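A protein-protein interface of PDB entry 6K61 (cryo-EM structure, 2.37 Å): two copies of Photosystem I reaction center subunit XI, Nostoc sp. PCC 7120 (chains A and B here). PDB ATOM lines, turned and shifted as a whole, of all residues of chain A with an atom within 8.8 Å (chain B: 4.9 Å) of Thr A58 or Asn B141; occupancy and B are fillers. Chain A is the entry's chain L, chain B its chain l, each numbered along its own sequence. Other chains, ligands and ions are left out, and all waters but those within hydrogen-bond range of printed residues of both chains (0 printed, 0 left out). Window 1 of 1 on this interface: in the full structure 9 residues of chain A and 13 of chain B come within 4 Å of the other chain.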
ATOM      1  N   PRO A  51     -16.993 -19.437   4.458  1.00  0.00           N
ATOM      2  CA  PRO A  51     -15.997 -19.507   3.378  1.00  0.00           C
ATOM      3  C   PRO A  51     -16.450 -20.221   2.131  1.00  0.00           C
ATOM      4  O   PRO A  51     -15.817 -20.044   1.093  1.00  0.00           O
ATOM      5  CB  PRO A  51     -14.829 -20.241   4.037  1.00  0.00           C
ATOM      6  CG  PRO A  51     -15.430 -20.961   5.157  1.00  0.00           C
ATOM      7  CD  PRO A  51     -16.525 -20.113   5.671  1.00  0.00           C
ATOM      8  N   ALA A  52     -17.533 -20.996   2.191  1.00  0.00           N
ATOM      9  CA  ALA A  52     -18.161 -21.505   0.983  1.00  0.00           C
ATOM     10  C   ALA A  52     -18.681 -20.382   0.100  1.00  0.00           C
ATOM     11  O   ALA A  52     -18.666 -20.502  -1.127  1.00  0.00           O
ATOM     12  CB  ALA A  52     -19.304 -22.449   1.350  1.00  0.00           C
ATOM     13  N   ARG A  54     -18.083 -16.680   0.796  1.00  0.00           N
ATOM     14  CA  ARG A  54     -17.545 -15.345   1.051  1.00  0.00           C
ATOM     15  C   ARG A  54     -16.899 -14.780  -0.206  1.00  0.00           C
ATOM     16  O   ARG A  54     -16.097 -15.464  -0.843  1.00  0.00           O
ATOM     17  CB  ARG A  54     -16.507 -15.368   2.158  1.00  0.00           C
ATOM     18  CG  ARG A  54     -16.203 -13.996   2.708  1.00  0.00           C
ATOM     19  CD  ARG A  54     -15.123 -13.996   3.761  1.00  0.00           C
ATOM     20  NE  ARG A  54     -15.432 -14.974   4.780  1.00  0.00           N
ATOM     21  CZ  ARG A  54     -14.624 -15.959   5.122  1.00  0.00           C
ATOM     22  NH1 ARG A  54     -13.433 -16.070   4.569  1.00  0.00           N
ATOM     23  NH2 ARG A  54     -15.008 -16.830   6.024  1.00  0.00           N
ATOM     24  N   PRO A  55     -17.213 -13.547  -0.584  1.00  0.00           N
ATOM     25  CA  PRO A  55     -16.569 -12.941  -1.750  1.00  0.00           C
ATOM     26  C   PRO A  55     -15.089 -12.675  -1.536  1.00  0.00           C
ATOM     27  O   PRO A  55     -14.616 -12.477  -0.417  1.00  0.00           O
ATOM     28  CB  PRO A  55     -17.337 -11.632  -1.929  1.00  0.00           C
ATOM     29  CG  PRO A  55     -17.893 -11.348  -0.594  1.00  0.00           C
ATOM     30  CD  PRO A  55     -18.234 -12.664  -0.003  1.00  0.00           C
ATOM     31  N   GLY A  56     -14.355 -12.680  -2.639  1.00  0.00           N
ATOM     32  CA  GLY A  56     -12.940 -12.391  -2.590  1.00  0.00           C
ATOM     33  C   GLY A  56     -12.063 -13.543  -2.172  1.00  0.00           C
ATOM     34  O   GLY A  56     -11.017 -13.316  -1.563  1.00  0.00           O
ATOM     35  N   LEU A  57     -12.450 -14.775  -2.480  1.00  0.00           N
ATOM     36  CA  LEU A  57     -11.652 -15.936  -2.126  1.00  0.00           C
ATOM     37  C   LEU A  57     -11.395 -16.782  -3.360  1.00  0.00           C
ATOM     38  O   LEU A  57     -12.286 -16.973  -4.190  1.00  0.00           O
ATOM     39  CB  LEU A  57     -12.337 -16.796  -1.065  1.00  0.00           C
ATOM     40  CG  LEU A  57     -12.745 -16.167   0.268  1.00  0.00           C
ATOM     41  CD1 LEU A  57     -13.347 -17.204   1.171  1.00  0.00           C
ATOM     42  CD2 LEU A  57     -11.600 -15.474   0.950  1.00  0.00           C
ATOM     43  N   THR A  58     -10.178 -17.278  -3.485  1.00  0.00           N
ATOM     44  CA  THR A  58      -9.859 -18.285  -4.479  1.00  0.00           C
ATOM     45  C   THR A  58     -10.389 -19.638  -3.992  1.00  0.00           C
ATOM     46  O   THR A  58     -10.734 -19.774  -2.817  1.00  0.00           O
ATOM     47  CB  THR A  58      -8.350 -18.308  -4.715  1.00  0.00           C
ATOM     48  OG1 THR A  58      -7.683 -18.765  -3.539  1.00  0.00           O
ATOM     49  CG2 THR A  58      -7.851 -16.918  -5.063  1.00  0.00           C
ATOM     50  N   PRO A  59     -10.549 -20.630  -4.888  1.00  0.00           N
ATOM     51  CA  PRO A  59     -11.017 -21.955  -4.428  1.00  0.00           C
ATOM     52  C   PRO A  59     -10.104 -22.631  -3.420  1.00  0.00           C
ATOM     53  O   PRO A  59     -10.598 -23.331  -2.528  1.00  0.00           O
ATOM     54  CB  PRO A  59     -11.100 -22.757  -5.731  1.00  0.00           C
ATOM     55  CG  PRO A  59     -11.327 -21.768  -6.761  1.00  0.00           C
ATOM     56  CD  PRO A  59     -10.601 -20.539  -6.361  1.00  0.00           C
ATOM     57  N   PHE A  60      -8.791 -22.412  -3.528  1.00  0.00           N
ATOM     58  CA  PHE A  60      -7.853 -22.905  -2.530  1.00  0.00           C
ATOM     59  C   PHE A  60      -8.107 -22.281  -1.160  1.00  0.00           C
ATOM     60  O   PHE A  60      -8.045 -22.965  -0.142  1.00  0.00           O
ATOM     61  CB  PHE A  60      -6.416 -22.624  -2.975  1.00  0.00           C
ATOM     62  CG  PHE A  60      -5.379 -23.172  -2.041  1.00  0.00           C
ATOM     63  CD1 PHE A  60      -4.987 -24.486  -2.134  1.00  0.00           C
ATOM     64  CD2 PHE A  60      -4.805 -22.381  -1.058  1.00  0.00           C
ATOM     65  CE1 PHE A  60      -4.065 -25.003  -1.270  1.00  0.00           C
ATOM     66  CE2 PHE A  60      -3.889 -22.900  -0.187  1.00  0.00           C
ATOM     67  CZ  PHE A  60      -3.513 -24.211  -0.298  1.00  0.00           C
ATOM     68  N   ARG A  61      -8.368 -20.978  -1.109  1.00  0.00           N
ATOM     69  CA  ARG A  61      -8.574 -20.319   0.174  1.00  0.00           C
ATOM     70  C   ARG A  61      -9.860 -20.802   0.858  1.00  0.00           C
ATOM     71  O   ARG A  61      -9.869 -21.051   2.077  1.00  0.00           O
ATOM     72  CB  ARG A  61      -8.549 -18.807  -0.061  1.00  0.00           C
ATOM     73  CG  ARG A  61      -8.887 -17.928   1.101  1.00  0.00           C
ATOM     74  CD  ARG A  61      -7.954 -18.062   2.280  1.00  0.00           C
ATOM     75  NE  ARG A  61      -8.368 -17.180   3.367  1.00  0.00           N
ATOM     76  CZ  ARG A  61      -9.312 -17.495   4.248  1.00  0.00           C
ATOM     77  NH1 ARG A  61      -9.659 -16.665   5.214  1.00  0.00           N
ATOM     78  NH2 ARG A  61      -9.926 -18.650   4.147  1.00  0.00           N
ATOM     79  N   ARG A  62     -10.911 -21.052   0.065  1.00  0.00           N
ATOM     80  CA  ARG A  62     -12.161 -21.604   0.586  1.00  0.00           C
ATOM     81  C   ARG A  62     -11.963 -23.013   1.126  1.00  0.00           C
ATOM     82  O   ARG A  62     -12.406 -23.335   2.238  1.00  0.00           O
ATOM     83  CB  ARG A  62     -13.227 -21.640  -0.506  1.00  0.00           C
ATOM     84  CG  ARG A  62     -13.534 -20.334  -1.135  1.00  0.00           C
ATOM     85  CD  ARG A  62     -14.702 -20.417  -2.064  1.00  0.00           C
ATOM     86  NE  ARG A  62     -14.915 -19.159  -2.757  1.00  0.00           N
ATOM     87  CZ  ARG A  62     -15.654 -18.168  -2.288  1.00  0.00           C
ATOM     88  NH1 ARG A  62     -16.261 -18.286  -1.123  1.00  0.00           N
ATOM     89  NH2 ARG A  62     -15.796 -17.061  -2.988  1.00  0.00           N
ATOM     90  N   GLY A  63     -11.339 -23.876   0.324  1.00  0.00           N
ATOM     91  CA  GLY A  63     -11.092 -25.238   0.749  1.00  0.00           C
ATOM     92  C   GLY A  63     -10.190 -25.336   1.951  1.00  0.00           C
ATOM     93  O   GLY A  63     -10.403 -26.189   2.805  1.00  0.00           O
ATOM     94  N   LEU A  64      -9.242 -24.413   2.077  1.00  0.00           N
ATOM     95  CA  LEU A  64      -8.321 -24.422   3.200  1.00  0.00           C
ATOM     96  C   LEU A  64      -9.027 -24.067   4.501  1.00  0.00           C
ATOM     97  O   LEU A  64      -8.839 -24.748   5.515  1.00  0.00           O
ATOM     98  CB  LEU A  64      -7.156 -23.485   2.878  1.00  0.00           C
ATOM     99  CG  LEU A  64      -5.814 -23.337   3.598  1.00  0.00           C
ATOM    100  CD1 LEU A  64      -5.893 -22.326   4.673  1.00  0.00           C
ATOM    101  CD2 LEU A  64      -5.336 -24.664   4.159  1.00  0.00           C
ATOM    102  N   GLU A  65      -9.906 -23.066   4.478  1.00  0.00           N
ATOM    103  CA  GLU A  65     -10.602 -22.716   5.716  1.00  0.00           C
ATOM    104  C   GLU A  65     -11.658 -23.755   6.113  1.00  0.00           C
ATOM    105  O   GLU A  65     -11.759 -24.123   7.299  1.00  0.00           O
ATOM    106  CB  GLU A  65     -11.212 -21.338   5.569  1.00  0.00           C
ATOM    107  CG  GLU A  65     -12.007 -20.898   6.743  1.00  0.00           C
ATOM    108  CD  GLU A  65     -12.485 -19.497   6.611  1.00  0.00           C
ATOM    109  OE1 GLU A  65     -11.950 -18.717   5.827  1.00  0.00           O
ATOM    110  OE2 GLU A  65     -13.513 -19.213   7.200  1.00  0.00           O
ATOM    111  N   PRO A 130     -20.327 -18.729  -5.577  1.00  0.00           N
ATOM    112  CA  PRO A 130     -19.084 -18.417  -6.286  1.00  0.00           C
ATOM    113  C   PRO A 130     -18.899 -19.281  -7.521  1.00  0.00           C
ATOM    114  O   PRO A 130     -19.442 -20.379  -7.640  1.00  0.00           O
ATOM    115  CB  PRO A 130     -18.002 -18.717  -5.248  1.00  0.00           C
ATOM    116  CG  PRO A 130     -18.699 -18.665  -3.961  1.00  0.00           C
ATOM    117  CD  PRO A 130     -20.052 -19.193  -4.209  1.00  0.00           C
ATOM    118  N   ASP A 131     -18.083 -18.767  -8.446  1.00  0.00           N
ATOM    119  CA  ASP A 131     -17.724 -19.504  -9.649  1.00  0.00           C
ATOM    120  C   ASP A 131     -16.761 -20.648  -9.377  1.00  0.00           C
ATOM    121  O   ASP A 131     -16.471 -21.415 -10.299  1.00  0.00           O
ATOM    122  CB  ASP A 131     -17.104 -18.573 -10.685  1.00  0.00           C
ATOM    123  CG  ASP A 131     -18.081 -17.547 -11.203  1.00  0.00           C
ATOM    124  OD1 ASP A 131     -19.301 -17.814 -11.183  1.00  0.00           O
ATOM    125  OD2 ASP A 131     -17.623 -16.472 -11.641  1.00  0.00           O
ATOM    126  N   ALA A 132     -16.253 -20.758  -8.147  1.00  0.00           N
ATOM    127  CA  ALA A 132     -15.396 -21.871  -7.763  1.00  0.00           C
ATOM    128  C   ALA A 132     -16.120 -23.202  -7.894  1.00  0.00           C
ATOM    129  O   ALA A 132     -15.527 -24.201  -8.302  1.00  0.00           O
ATOM    130  CB  ALA A 132     -14.923 -21.680  -6.325  1.00  0.00           C
ATOM    131  N   PHE A 133     -17.407 -23.238  -7.567  1.00  0.00           N
ATOM    132  CA  PHE A 133     -18.140 -24.492  -7.525  1.00  0.00           C
ATOM    133  C   PHE A 133     -18.953 -24.720  -8.791  1.00  0.00           C
ATOM    134  O   PHE A 133     -19.975 -25.408  -8.762  1.00  0.00           O
ATOM    135  CB  PHE A 133     -19.016 -24.517  -6.277  1.00  0.00           C
ATOM    136  CG  PHE A 133     -18.252 -24.235  -5.017  1.00  0.00           C
ATOM    137  CD1 PHE A 133     -17.360 -25.162  -4.512  1.00  0.00           C
ATOM    138  CD2 PHE A 133     -18.418 -23.038  -4.341  1.00  0.00           C
ATOM    139  CE1 PHE A 133     -16.653 -24.902  -3.362  1.00  0.00           C
ATOM    140  CE2 PHE A 133     -17.717 -22.782  -3.187  1.00  0.00           C
ATOM    141  CZ  PHE A 133     -16.831 -23.709  -2.701  1.00  0.00           C
ATOM    142  N   GLY A 138     -12.227 -25.770 -10.124  1.00  0.00           N
ATOM    143  CA  GLY A 138     -12.485 -25.141  -8.843  1.00  0.00           C
ATOM    144  C   GLY A 138     -12.740 -26.155  -7.748  1.00  0.00           C
ATOM    145  O   GLY A 138     -12.260 -25.995  -6.623  1.00  0.00           O
ATOM    146  N   ASN A 141      -9.232 -27.787  -6.942  1.00  0.00           N
ATOM    147  CA  ASN A 141      -8.455 -26.889  -6.096  1.00  0.00           C
ATOM    148  C   ASN A 141      -8.998 -26.875  -4.677  1.00  0.00           C
ATOM    149  O   ASN A 141      -8.224 -26.900  -3.709  1.00  0.00           O
ATOM    150  CB  ASN A 141      -8.471 -25.471  -6.662  1.00  0.00           C
ATOM    151  CG  ASN A 141      -7.722 -25.346  -7.967  1.00  0.00           C
ATOM    152  OD1 ASN A 141      -6.684 -25.968  -8.168  1.00  0.00           O
ATOM    153  ND2 ASN A 141      -8.227 -24.502  -8.850  1.00  0.00           N
ATOM    154  N   PHE A 142     -10.330 -26.870  -4.548  1.00  0.00           N
ATOM    155  CA  PHE A 142     -10.992 -26.931  -3.252  1.00  0.00           C
ATOM    156  C   PHE A 142     -10.596 -28.190  -2.490  1.00  0.00           C
ATOM    157  O   PHE A 142     -10.313 -28.129  -1.296  1.00  0.00           O
ATOM    158  CB  PHE A 142     -12.506 -26.886  -3.459  1.00  0.00           C
ATOM    159  CG  PHE A 142     -13.307 -26.755  -2.201  1.00  0.00           C
ATOM    160  CD1 PHE A 142     -13.611 -25.510  -1.698  1.00  0.00           C
ATOM    161  CD2 PHE A 142     -13.763 -27.872  -1.524  1.00  0.00           C
ATOM    162  CE1 PHE A 142     -14.352 -25.376  -0.561  1.00  0.00           C
ATOM    163  CE2 PHE A 142     -14.491 -27.737  -0.374  1.00  0.00           C
ATOM    164  CZ  PHE A 142     -14.779 -26.485   0.109  1.00  0.00           C
ATOM    165  N   ALA A 145      -7.045 -28.206  -1.293  1.00  0.00           N
ATOM    166  CA  ALA A 145      -6.951 -27.337  -0.131  1.00  0.00           C
ATOM    167  C   ALA A 145      -7.595 -27.953   1.100  1.00  0.00           C
ATOM    168  O   ALA A 145      -7.124 -27.744   2.223  1.00  0.00           O
ATOM    169  CB  ALA A 145      -7.635 -26.038  -0.450  1.00  0.00           C
ATOM    170  N   PRO B  59       0.734 -15.554  -4.568  1.00  0.00           N
ATOM    171  CA  PRO B  59       0.471 -14.996  -3.220  1.00  0.00           C
ATOM    172  C   PRO B  59       0.671 -15.966  -2.067  1.00  0.00           C
ATOM    173  O   PRO B  59       1.132 -15.558  -0.993  1.00  0.00           O
ATOM    174  CB  PRO B  59      -0.994 -14.557  -3.320  1.00  0.00           C
ATOM    175  CG  PRO B  59      -1.195 -14.253  -4.724  1.00  0.00           C
ATOM    176  CD  PRO B  59      -0.336 -15.180  -5.516  1.00  0.00           C
ATOM    177  N   PHE B  60       0.400 -17.253  -2.282  1.00  0.00           N
ATOM    178  CA  PHE B  60       0.608 -18.233  -1.228  1.00  0.00           C
ATOM    179  C   PHE B  60       2.094 -18.476  -0.984  1.00  0.00           C
ATOM    180  O   PHE B  60       2.518 -18.668   0.155  1.00  0.00           O
ATOM    181  CB  PHE B  60      -0.098 -19.547  -1.570  1.00  0.00           C
ATOM    182  CG  PHE B  60      -0.236 -20.483  -0.402  1.00  0.00           C
ATOM    183  CD1 PHE B  60      -1.336 -20.414   0.420  1.00  0.00           C
ATOM    184  CD2 PHE B  60       0.758 -21.403  -0.102  1.00  0.00           C
ATOM    185  CE1 PHE B  60      -1.458 -21.245   1.498  1.00  0.00           C
ATOM    186  CE2 PHE B  60       0.642 -22.227   0.983  1.00  0.00           C
ATOM    187  CZ  PHE B  60      -0.474 -22.153   1.781  1.00  0.00           C
ATOM    188  N   GLU B 137      -8.339 -11.214  -3.440  1.00  0.00           N
ATOM    189  CA  GLU B 137      -8.047 -12.644  -3.461  1.00  0.00           C
ATOM    190  C   GLU B 137      -6.574 -12.921  -3.205  1.00  0.00           C
ATOM    191  O   GLU B 137      -6.232 -13.869  -2.484  1.00  0.00           O
ATOM    192  CB  GLU B 137      -8.465 -13.248  -4.798  1.00  0.00           C
ATOM    193  CG  GLU B 137      -9.955 -13.248  -5.040  1.00  0.00           C
ATOM    194  CD  GLU B 137     -10.335 -13.957  -6.321  1.00  0.00           C
ATOM    195  OE1 GLU B 137      -9.427 -14.318  -7.095  1.00  0.00           O
ATOM    196  OE2 GLU B 137     -11.543 -14.172  -6.556  1.00  0.00           O
ATOM    197  N   GLY B 138      -5.690 -12.117  -3.801  1.00  0.00           N
ATOM    198  CA  GLY B 138      -4.268 -12.248  -3.537  1.00  0.00           C
ATOM    199  C   GLY B 138      -3.910 -11.961  -2.093  1.00  0.00           C
ATOM    200  O   GLY B 138      -3.089 -12.656  -1.505  1.00  0.00           O
ATOM    201  N   TRP B 139      -4.588 -10.993  -1.476  1.00  0.00           N
ATOM    202  CA  TRP B 139      -4.331 -10.714  -0.069  1.00  0.00           C
ATOM    203  C   TRP B 139      -4.896 -11.796   0.842  1.00  0.00           C
ATOM    204  O   TRP B 139      -4.308 -12.089   1.886  1.00  0.00           O
ATOM    205  CB  TRP B 139      -4.879  -9.349   0.329  1.00  0.00           C
ATOM    206  CG  TRP B 139      -4.049  -8.184  -0.013  1.00  0.00           C
ATOM    207  CD1 TRP B 139      -4.261  -7.294  -1.011  1.00  0.00           C
ATOM    208  CD2 TRP B 139      -2.876  -7.749   0.671  1.00  0.00           C
ATOM    209  NE1 TRP B 139      -3.291  -6.338  -0.998  1.00  0.00           N
ATOM    210  CE2 TRP B 139      -2.419  -6.601   0.021  1.00  0.00           C
ATOM    211  CE3 TRP B 139      -2.155  -8.242   1.761  1.00  0.00           C
ATOM    212  CZ2 TRP B 139      -1.277  -5.927   0.426  1.00  0.00           C
ATOM    213  CZ3 TRP B 139      -1.032  -7.583   2.159  1.00  0.00           C
ATOM    214  CH2 TRP B 139      -0.599  -6.431   1.495  1.00  0.00           C
ATOM    215  N   ASN B 140      -6.009 -12.431   0.450  1.00  0.00           N
ATOM    216  CA  ASN B 140      -6.524 -13.551   1.236  1.00  0.00           C
ATOM    217  C   ASN B 140      -5.599 -14.763   1.150  1.00  0.00           C
ATOM    218  O   ASN B 140      -5.368 -15.451   2.155  1.00  0.00           O
ATOM    219  CB  ASN B 140      -7.930 -13.927   0.779  1.00  0.00           C
ATOM    220  CG  ASN B 140      -8.972 -12.905   1.181  1.00  0.00           C
ATOM    221  OD1 ASN B 140      -9.047 -12.496   2.331  1.00  0.00           O
ATOM    222  ND2 ASN B 140      -9.749 -12.459   0.222  1.00  0.00           N
ATOM    223  N   ASN B 141      -5.008 -14.965  -0.017  1.00  0.00           N
ATOM    224  CA  ASN B 141      -4.066 -16.046  -0.211  1.00  0.00           C
ATOM    225  C   ASN B 141      -2.826 -15.789   0.618  1.00  0.00           C
ATOM    226  O   ASN B 141      -2.344 -16.668   1.299  1.00  0.00           O
ATOM    227  CB  ASN B 141      -3.697 -16.168  -1.673  1.00  0.00           C
ATOM    228  CG  ASN B 141      -4.420 -17.293  -2.351  1.00  0.00           C
ATOM    229  OD1 ASN B 141      -3.820 -18.297  -2.720  1.00  0.00           O
ATOM    230  ND2 ASN B 141      -5.716 -17.139  -2.515  1.00  0.00           N
ATOM    231  N   PHE B 142      -2.313 -14.570   0.536  1.00  0.00           N
ATOM    232  CA  PHE B 142      -1.163 -14.143   1.322  1.00  0.00           C
ATOM    233  C   PHE B 142      -1.411 -14.340   2.807  1.00  0.00           C
ATOM    234  O   PHE B 142      -0.546 -14.860   3.508  1.00  0.00           O
ATOM    235  CB  PHE B 142      -0.831 -12.674   1.031  1.00  0.00           C
ATOM    236  CG  PHE B 142       0.403 -12.168   1.734  1.00  0.00           C
ATOM    237  CD1 PHE B 142       1.650 -12.376   1.194  1.00  0.00           C
ATOM    238  CD2 PHE B 142       0.309 -11.480   2.926  1.00  0.00           C
ATOM    239  CE1 PHE B 142       2.775 -11.908   1.825  1.00  0.00           C
ATOM    240  CE2 PHE B 142       1.429 -11.029   3.560  1.00  0.00           C
ATOM    241  CZ  PHE B 142       2.665 -11.238   3.009  1.00  0.00           C
ATOM    242  N   ALA B 143      -2.597 -13.966   3.294  1.00  0.00           N
ATOM    243  CA  ALA B 143      -2.885 -14.025   4.724  1.00  0.00           C
ATOM    244  C   ALA B 143      -2.974 -15.457   5.237  1.00  0.00           C
ATOM    245  O   ALA B 143      -2.440 -15.772   6.310  1.00  0.00           O
ATOM    246  CB  ALA B 143      -4.181 -13.290   5.026  1.00  0.00           C
ATOM    247  N   SER B 144      -3.640 -16.339   4.486  1.00  0.00           N
ATOM    248  CA  SER B 144      -3.710 -17.742   4.895  1.00  0.00           C
ATOM    249  C   SER B 144      -2.336 -18.402   4.855  1.00  0.00           C
ATOM    250  O   SER B 144      -1.987 -19.197   5.745  1.00  0.00           O
ATOM    251  CB  SER B 144      -4.711 -18.493   4.020  1.00  0.00           C
ATOM    252  OG  SER B 144      -4.354 -18.516   2.656  1.00  0.00           O
ATOM    253  N   ALA B 145      -1.521 -18.030   3.870  1.00  0.00           N
ATOM    254  CA  ALA B 145      -0.161 -18.535   3.799  1.00  0.00           C
ATOM    255  C   ALA B 145       0.683 -18.017   4.947  1.00  0.00           C
ATOM    256  O   ALA B 145       1.563 -18.722   5.444  1.00  0.00           O
ATOM    257  CB  ALA B 145       0.450 -18.125   2.479  1.00  0.00           C
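O of Gly A56 sits close to ND2 of Asn B140.
The side-chain amide nitrogen (ND2) of Asn B141 sits at hydrogen-bond distance from the side-chain hydroxyl (OG1) of Thr A58 (2.7 Å).
The backbone carbonyl oxygen (O) of Asn B140 lies within hydrogen-bond range of the side-chain hydroxyl (OG) of Ser B144, 3.3 Å away.
O of Glu B137 sits at hydrogen-bond distance from ND2 of Asn B141 (3.3 Å).
The side-chain hydroxyl (OG1) of Thr A58 is in hydrogen-bond range of the backbone NH (N) of Arg A61 (3.4 Å).
O of Asn B141 is in hydrogen-bond range of OG of Ser B144.
OE1 of Glu A65 lies within salt-bridge range of NH2 of Arg A61 (2.6 Å).
Gly A56 touches Glu B137.
Leu A57 touches Glu B137.
ND2 of Asn B140 touches CD2 of Leu A57 (3.6 Å).
Thr A58 touches Glu B137.
CE2 of Phe A60 touches CE1 of Phe B60, at 3.4 Å.
Arg A61 touches Asn B140.
Arg A61 touches Ser B144 (CD to OG, 3.6 Å).
Thr A58 touches just these residues of chain B: Glu B137 (3.7 Å) and Asn B141 (2.7 Å).
Of chain A, only Thr A58 (2.7 Å) comes within 4 Å of Asn B141.
Printed residues of chain B within 4 Å of Arg A61: Asn B140 (3.7 Å) and Ser B144 (3.6 Å).
Of the printed residues of chain A, Phe B60 touches Phe A60.
Of the printed residues of chain B, Phe A60 touches Phe B60.
Printed residues of chain B within 4 Å of Gly A56: Glu B137 (3.6 Å) and Asn B140 (2.4 Å).
The nearest printed residue of chain B that does not touch Thr A58 is Gly B138 (5.4 Å).
The nearest residue of chain A that does not touch Asn B141 is Arg A61 (4.1 Å).
Hydrophobic or aromatic side chains of chain B that line the printed part of chain A: Phe B60.
Among the printed residues, 9 pairs touch across the chains.
Among the printed residues, no Asp or Glu carboxylate lies within 4 Å of a Lys or Arg side-chain nitrogen of the other chain.
Phe B60 touches its own counterpart, Phe A60.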
